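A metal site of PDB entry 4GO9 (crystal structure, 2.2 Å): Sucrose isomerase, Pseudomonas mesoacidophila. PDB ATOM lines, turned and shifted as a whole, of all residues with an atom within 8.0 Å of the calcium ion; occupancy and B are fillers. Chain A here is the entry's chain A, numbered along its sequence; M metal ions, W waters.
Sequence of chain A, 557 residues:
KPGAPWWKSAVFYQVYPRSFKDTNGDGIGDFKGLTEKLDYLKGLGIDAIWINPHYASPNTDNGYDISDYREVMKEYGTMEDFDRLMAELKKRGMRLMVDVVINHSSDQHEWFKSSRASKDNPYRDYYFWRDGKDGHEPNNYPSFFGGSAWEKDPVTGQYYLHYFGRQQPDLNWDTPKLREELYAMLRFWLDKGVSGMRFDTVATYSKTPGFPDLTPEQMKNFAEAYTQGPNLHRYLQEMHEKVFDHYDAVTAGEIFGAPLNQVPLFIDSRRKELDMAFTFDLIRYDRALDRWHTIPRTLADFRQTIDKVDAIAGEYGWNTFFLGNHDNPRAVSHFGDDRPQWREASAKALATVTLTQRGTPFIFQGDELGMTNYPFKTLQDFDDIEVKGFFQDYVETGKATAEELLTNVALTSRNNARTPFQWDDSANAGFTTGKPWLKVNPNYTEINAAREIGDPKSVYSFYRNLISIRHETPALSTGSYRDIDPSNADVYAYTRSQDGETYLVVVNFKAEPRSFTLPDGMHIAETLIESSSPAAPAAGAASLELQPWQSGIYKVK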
ATOM      1  N   PRO A  17      16.184  23.221  21.553  1.00  0.00           N
ATOM      2  CA  PRO A  17      15.754  22.022  20.824  1.00  0.00           C
ATOM      3  C   PRO A  17      16.235  21.981  19.369  1.00  0.00           C
ATOM      4  O   PRO A  17      16.514  20.899  18.850  1.00  0.00           O
ATOM      5  CB  PRO A  17      14.226  22.118  20.871  1.00  0.00           C
ATOM      6  CG  PRO A  17      13.943  22.886  22.107  1.00  0.00           C
ATOM      7  CD  PRO A  17      15.041  23.913  22.179  1.00  0.00           C
ATOM      8  N   ARG A  18      16.331  23.136  18.728  1.00  0.00           N
ATOM      9  CA  ARG A  18      16.754  23.211  17.336  1.00  0.00           C
ATOM     10  C   ARG A  18      18.158  22.647  17.131  1.00  0.00           C
ATOM     11  O   ARG A  18      18.474  22.106  16.071  1.00  0.00           O
ATOM     12  CB  ARG A  18      16.679  24.662  16.838  1.00  0.00           C
ATOM     13  CG  ARG A  18      16.904  24.823  15.345  1.00  0.00           C
ATOM     14  CD  ARG A  18      16.848  26.289  14.939  1.00  0.00           C
ATOM     15  NE  ARG A  18      16.998  26.432  13.494  1.00  0.00           N
ATOM     16  CZ  ARG A  18      15.987  26.356  12.632  1.00  0.00           C
ATOM     17  NH1 ARG A  18      14.753  26.140  13.073  1.00  0.00           N
ATOM     18  NH2 ARG A  18      16.207  26.506  11.325  1.00  0.00           N
ATOM     19  N   LYS A  21      19.277  17.610  19.564  1.00  0.00           N
ATOM     20  CA  LYS A  21      19.374  16.262  19.003  1.00  0.00           C
ATOM     21  C   LYS A  21      18.350  15.993  17.906  1.00  0.00           C
ATOM     22  O   LYS A  21      17.148  16.066  18.141  1.00  0.00           O
ATOM     23  CB  LYS A  21      19.270  15.197  20.097  1.00  0.00           C
ATOM     24  CG  LYS A  21      19.415  13.761  19.602  1.00  0.00           C
ATOM     25  CD  LYS A  21      20.733  13.570  18.853  1.00  0.00           C
ATOM     26  CE  LYS A  21      21.063  12.093  18.677  1.00  0.00           C
ATOM     27  NZ  LYS A  21      19.995  11.323  17.979  1.00  0.00           N
ATOM     28  N   ASP A  22      18.843  15.677  16.713  1.00  0.00           N
ATOM     29  CA  ASP A  22      18.013  15.399  15.548  1.00  0.00           C
ATOM     30  C   ASP A  22      17.843  13.893  15.373  1.00  0.00           C
ATOM     31  O   ASP A  22      18.822  13.141  15.497  1.00  0.00           O
ATOM     32  CB  ASP A  22      18.635  16.030  14.299  1.00  0.00           C
ATOM     33  CG  ASP A  22      17.876  15.702  13.027  1.00  0.00           C
ATOM     34  OD1 ASP A  22      16.667  15.399  13.102  1.00  0.00           O
ATOM     35  OD2 ASP A  22      18.493  15.768  11.938  1.00  0.00           O
ATOM     36  N   THR A  23      16.623  13.443  15.087  1.00  0.00           N
ATOM     37  CA  THR A  23      16.350  12.014  14.990  1.00  0.00           C
ATOM     38  C   THR A  23      15.738  11.581  13.651  1.00  0.00           C
ATOM     39  O   THR A  23      15.395  10.415  13.485  1.00  0.00           O
ATOM     40  CB  THR A  23      15.419  11.522  16.120  1.00  0.00           C
ATOM     41  OG1 THR A  23      14.231  12.320  16.144  1.00  0.00           O
ATOM     42  CG2 THR A  23      16.119  11.609  17.464  1.00  0.00           C
ATOM     43  N   ASN A  24      15.598  12.504  12.709  1.00  0.00           N
ATOM     44  CA  ASN A  24      15.045  12.147  11.405  1.00  0.00           C
ATOM     45  C   ASN A  24      15.861  12.684  10.227  1.00  0.00           C
ATOM     46  O   ASN A  24      15.390  12.701   9.090  1.00  0.00           O
ATOM     47  CB  ASN A  24      13.583  12.561  11.288  1.00  0.00           C
ATOM     48  CG  ASN A  24      13.406  14.064  11.273  1.00  0.00           C
ATOM     49  OD1 ASN A  24      14.281  14.810  11.703  1.00  0.00           O
ATOM     50  ND2 ASN A  24      12.257  14.514  10.788  1.00  0.00           N
ATOM     51  N   GLY A  25      17.081  13.135  10.512  1.00  0.00           N
ATOM     52  CA  GLY A  25      18.030  13.507   9.487  1.00  0.00           C
ATOM     53  C   GLY A  25      17.764  14.785   8.714  1.00  0.00           C
ATOM     54  O   GLY A  25      18.398  15.026   7.685  1.00  0.00           O
ATOM     55  N   ASP A  26      16.835  15.613   9.195  1.00  0.00           N
ATOM     56  CA  ASP A  26      16.549  16.877   8.523  1.00  0.00           C
ATOM     57  C   ASP A  26      17.524  17.974   8.950  1.00  0.00           C
ATOM     58  O   ASP A  26      17.491  19.096   8.440  1.00  0.00           O
ATOM     59  CB  ASP A  26      15.091  17.313   8.732  1.00  0.00           C
ATOM     60  CG  ASP A  26      14.805  17.703  10.167  1.00  0.00           C
ATOM     61  OD1 ASP A  26      15.564  17.303  11.067  1.00  0.00           O
ATOM     62  OD2 ASP A  26      13.800  18.421  10.382  1.00  0.00           O
ATOM     63  N   GLY A  27      18.391  17.646   9.907  1.00  0.00           N
ATOM     64  CA  GLY A  27      19.423  18.561  10.357  1.00  0.00           C
ATOM     65  C   GLY A  27      18.970  19.482  11.475  1.00  0.00           C
ATOM     66  O   GLY A  27      19.738  20.319  11.956  1.00  0.00           O
ATOM     67  N   ILE A  28      17.718  19.320  11.895  1.00  0.00           N
ATOM     68  CA  ILE A  28      17.146  20.134  12.951  1.00  0.00           C
ATOM     69  C   ILE A  28      16.762  19.264  14.142  1.00  0.00           C
ATOM     70  O   ILE A  28      16.176  18.197  13.980  1.00  0.00           O
ATOM     71  CB  ILE A  28      15.930  20.931  12.438  1.00  0.00           C
ATOM     72  CG1 ILE A  28      16.366  21.954  11.402  1.00  0.00           C
ATOM     73  CG2 ILE A  28      15.203  21.610  13.581  1.00  0.00           C
ATOM     74  CD1 ILE A  28      15.224  22.690  10.727  1.00  0.00           C
ATOM     75  N   GLY A  29      17.118  19.698  15.347  1.00  0.00           N
ATOM     76  CA  GLY A  29      16.772  18.967  16.551  1.00  0.00           C
ATOM     77  C   GLY A  29      15.273  18.912  16.734  1.00  0.00           C
ATOM     78  O   GLY A  29      14.543  19.750  16.199  1.00  0.00           O
ATOM     79  N   ASP A  30      14.816  17.941  17.510  1.00  0.00           N
ATOM     80  CA  ASP A  30      13.382  17.707  17.673  1.00  0.00           C
ATOM     81  C   ASP A  30      13.057  17.138  19.058  1.00  0.00           C
ATOM     82  O   ASP A  30      13.949  16.934  19.884  1.00  0.00           O
ATOM     83  CB  ASP A  30      12.882  16.757  16.579  1.00  0.00           C
ATOM     84  CG  ASP A  30      13.790  15.550  16.404  1.00  0.00           C
ATOM     85  OD1 ASP A  30      13.826  14.685  17.299  1.00  0.00           O
ATOM     86  OD2 ASP A  30      14.472  15.471  15.356  1.00  0.00           O
ATOM     87  N   PHE A  31      11.777  16.886  19.298  1.00  0.00           N
ATOM     88  CA  PHE A  31      11.304  16.385  20.585  1.00  0.00           C
ATOM     89  C   PHE A  31      11.813  14.978  20.897  1.00  0.00           C
ATOM     90  O   PHE A  31      12.261  14.707  22.007  1.00  0.00           O
ATOM     91  CB  PHE A  31       9.782  16.402  20.646  1.00  0.00           C
ATOM     92  CG  PHE A  31       9.197  17.761  20.862  1.00  0.00           C
ATOM     93  CD1 PHE A  31       9.755  18.635  21.783  1.00  0.00           C
ATOM     94  CD2 PHE A  31       8.082  18.180  20.154  1.00  0.00           C
ATOM     95  CE1 PHE A  31       9.220  19.888  21.986  1.00  0.00           C
ATOM     96  CE2 PHE A  31       7.548  19.433  20.356  1.00  0.00           C
ATOM     97  CZ  PHE A  31       8.114  20.285  21.268  1.00  0.00           C
ATOM     98  N   LYS A  32      11.717  14.087  19.905  1.00  0.00           N
ATOM     99  CA  LYS A  32      12.215  12.725  20.051  1.00  0.00           C
ATOM    100  C   LYS A  32      13.685  12.743  20.438  1.00  0.00           C
ATOM    101  O   LYS A  32      14.129  11.901  21.218  1.00  0.00           O
ATOM    102  CB  LYS A  32      12.040  11.945  18.750  1.00  0.00           C
ATOM    103  CG  LYS A  32      10.628  11.470  18.473  1.00  0.00           C
ATOM    104  CD  LYS A  32      10.597  10.599  17.221  1.00  0.00           C
ATOM    105  CE  LYS A  32       9.216  10.047  16.942  1.00  0.00           C
ATOM    106  NZ  LYS A  32       9.211   9.136  15.763  1.00  0.00           N
ATOM    107  N   GLY A  33      14.428  13.698  19.881  1.00  0.00           N
ATOM    108  CA  GLY A  33      15.835  13.841  20.186  1.00  0.00           C
ATOM    109  C   GLY A  33      16.080  14.188  21.641  1.00  0.00           C
ATOM    110  O   GLY A  33      16.943  13.598  22.288  1.00  0.00           O
ATOM    111  N   LYS A  74       6.299  22.307  13.857  1.00  0.00           N
ATOM    112  CA  LYS A  74       6.350  21.182  12.928  1.00  0.00           C
ATOM    113  C   LYS A  74       7.706  20.507  12.935  1.00  0.00           C
ATOM    114  O   LYS A  74       7.803  19.275  12.885  1.00  0.00           O
ATOM    115  CB  LYS A  74       6.001  21.629  11.507  1.00  0.00           C
ATOM    116  N   GLU A  75       8.767  21.311  13.000  1.00  0.00           N
ATOM    117  CA  GLU A  75      10.128  20.795  13.006  1.00  0.00           C
ATOM    118  C   GLU A  75      10.390  19.872  14.192  1.00  0.00           C
ATOM    119  O   GLU A  75      11.089  18.876  14.057  1.00  0.00           O
ATOM    120  CB  GLU A  75      11.131  21.948  13.001  1.00  0.00           C
ATOM    121  CG  GLU A  75      11.412  22.552  11.628  1.00  0.00           C
ATOM    122  CD  GLU A  75      10.301  23.463  11.135  1.00  0.00           C
ATOM    123  OE1 GLU A  75       9.416  23.814  11.933  1.00  0.00           O
ATOM    124  OE2 GLU A  75      10.342  23.836   9.943  1.00  0.00           O
ATOM    125  N   TYR A  76       9.839  20.209  15.350  1.00  0.00           N
ATOM    126  CA  TYR A  76      10.163  19.479  16.576  1.00  0.00           C
ATOM    127  C   TYR A  76       9.342  18.196  16.743  1.00  0.00           C
ATOM    128  O   TYR A  76       9.722  17.302  17.505  1.00  0.00           O
ATOM    129  CB  TYR A  76      10.016  20.375  17.810  1.00  0.00           C
ATOM    130  CG  TYR A  76      10.919  21.595  17.787  1.00  0.00           C
ATOM    131  CD1 TYR A  76      12.017  21.664  16.935  1.00  0.00           C
ATOM    132  CD2 TYR A  76      10.667  22.682  18.626  1.00  0.00           C
ATOM    133  CE1 TYR A  76      12.832  22.769  16.919  1.00  0.00           C
ATOM    134  CE2 TYR A  76      11.488  23.798  18.604  1.00  0.00           C
ATOM    135  CZ  TYR A  76      12.564  23.839  17.749  1.00  0.00           C
ATOM    136  OH  TYR A  76      13.383  24.942  17.720  1.00  0.00           O
ATOM    137  N   GLY A  77       8.232  18.107  16.025  1.00  0.00           N
ATOM    138  CA  GLY A  77       7.393  16.922  16.083  1.00  0.00           C
ATOM    139  C   GLY A  77       5.915  17.245  16.237  1.00  0.00           C
ATOM    140  O   GLY A  77       5.439  18.241  15.707  1.00  0.00           O
ATOM    141  N   PHE A 431      24.945  14.517  16.149  1.00  0.00           N
ATOM    142  CA  PHE A 431      23.739  15.336  16.283  1.00  0.00           C
ATOM    143  C   PHE A 431      22.693  14.930  15.260  1.00  0.00           C
ATOM    144  O   PHE A 431      21.498  14.889  15.544  1.00  0.00           O
ATOM    145  CB  PHE A 431      24.083  16.823  16.139  1.00  0.00           C
ATOM    146  CG  PHE A 431      22.909  17.696  15.827  1.00  0.00           C
ATOM    147  CD1 PHE A 431      21.991  18.037  16.803  1.00  0.00           C
ATOM    148  CD2 PHE A 431      22.716  18.191  14.542  1.00  0.00           C
ATOM    149  CE1 PHE A 431      20.906  18.852  16.511  1.00  0.00           C
ATOM    150  CE2 PHE A 431      21.635  19.004  14.236  1.00  0.00           C
ATOM    151  CZ  PHE A 431      20.726  19.329  15.225  1.00  0.00           C
ATOM    152  N   THR A 432      23.154  14.642  14.039  1.00  0.00           N
ATOM    153  CA  THR A 432      22.249  14.299  12.950  1.00  0.00           C
ATOM    154  C   THR A 432      22.893  13.323  11.985  1.00  0.00           C
ATOM    155  O   THR A 432      24.120  13.193  11.937  1.00  0.00           O
ATOM    156  CB  THR A 432      21.825  15.556  12.165  1.00  0.00           C
ATOM    157  OG1 THR A 432      20.871  15.201  11.168  1.00  0.00           O
ATOM    158  CG2 THR A 432      23.027  16.209  11.498  1.00  0.00           C
HETATM  159 CA    CA M   1      14.645  16.621  13.160  1.00  0.00          CA
HETATM  160  O   HOH W   1      13.217  18.438  12.778  1.00  0.00           O
HETATM  161  O   HOH W   2      12.190  16.284  13.377  1.00  0.00           O
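Water W1 lies within hydrogen-bond range of the side-chain carboxylate of Asp 26 (2.5 Å) and the backbone carbonyl oxygen of Glu 75 (2.5 Å). Water W2 bridges the backbone carbonyl oxygen of Glu 75 (2.9 Å) and the side-chain amide nitrogen of Asn 24 (3.1 Å).
OD2 of Asp 22 is in hydrogen-bond range of N of Gly 25, at 3.3 Å. The side-chain carboxylate of Asp 22 lies within hydrogen-bond range of the backbone NH of Gly 27 (2.8 Å). The side-chain carboxylate (OD2) of Asp 22 is in hydrogen-bond range of the side-chain hydroxyl (OG1) of Thr 432, at 2.6 Å. The backbone NH (N) of Asp 22 lies within hydrogen-bond range of the backbone carbonyl oxygen (O) of Phe 431, at 3.0 Å. OD1 of Asp 30 lies within hydrogen-bond range of OG1 of Thr 23 (2.7 Å). O of Lys 21 lies within hydrogen-bond range of N of Asp 30, at 3.1 Å. The side-chain carboxylate (OD1) of Asp 30 is in hydrogen-bond range of the backbone NH (N) of Gly 33. The backbone NH (N) of Lys 32 sits at hydrogen-bond distance from the side-chain carboxylate (OD1) of Asp 30 (3.4 Å).
The calcium ion is bound by water W1 (2.3 Å), the backbone carbonyl oxygen (O) of Ile 28 (2.3 Å), the side-chain amide oxygen (OD1) of Asn 24 (2.4 Å), the side-chain carboxylate (OD1) of Asp 22 (2.4 Å), the side-chain carboxylate (OD1) of Asp 26 (2.4 Å), the side-chain carboxylate (OD2) of Asp 30 (2.5 Å) and water W2 (2.5 Å). The calcium ion has seven donor atoms within binding distance.
Within 4 Å of the calcium ion: Asp 22, Asn 24, Asp 26, Ile 28 and Asp 30.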
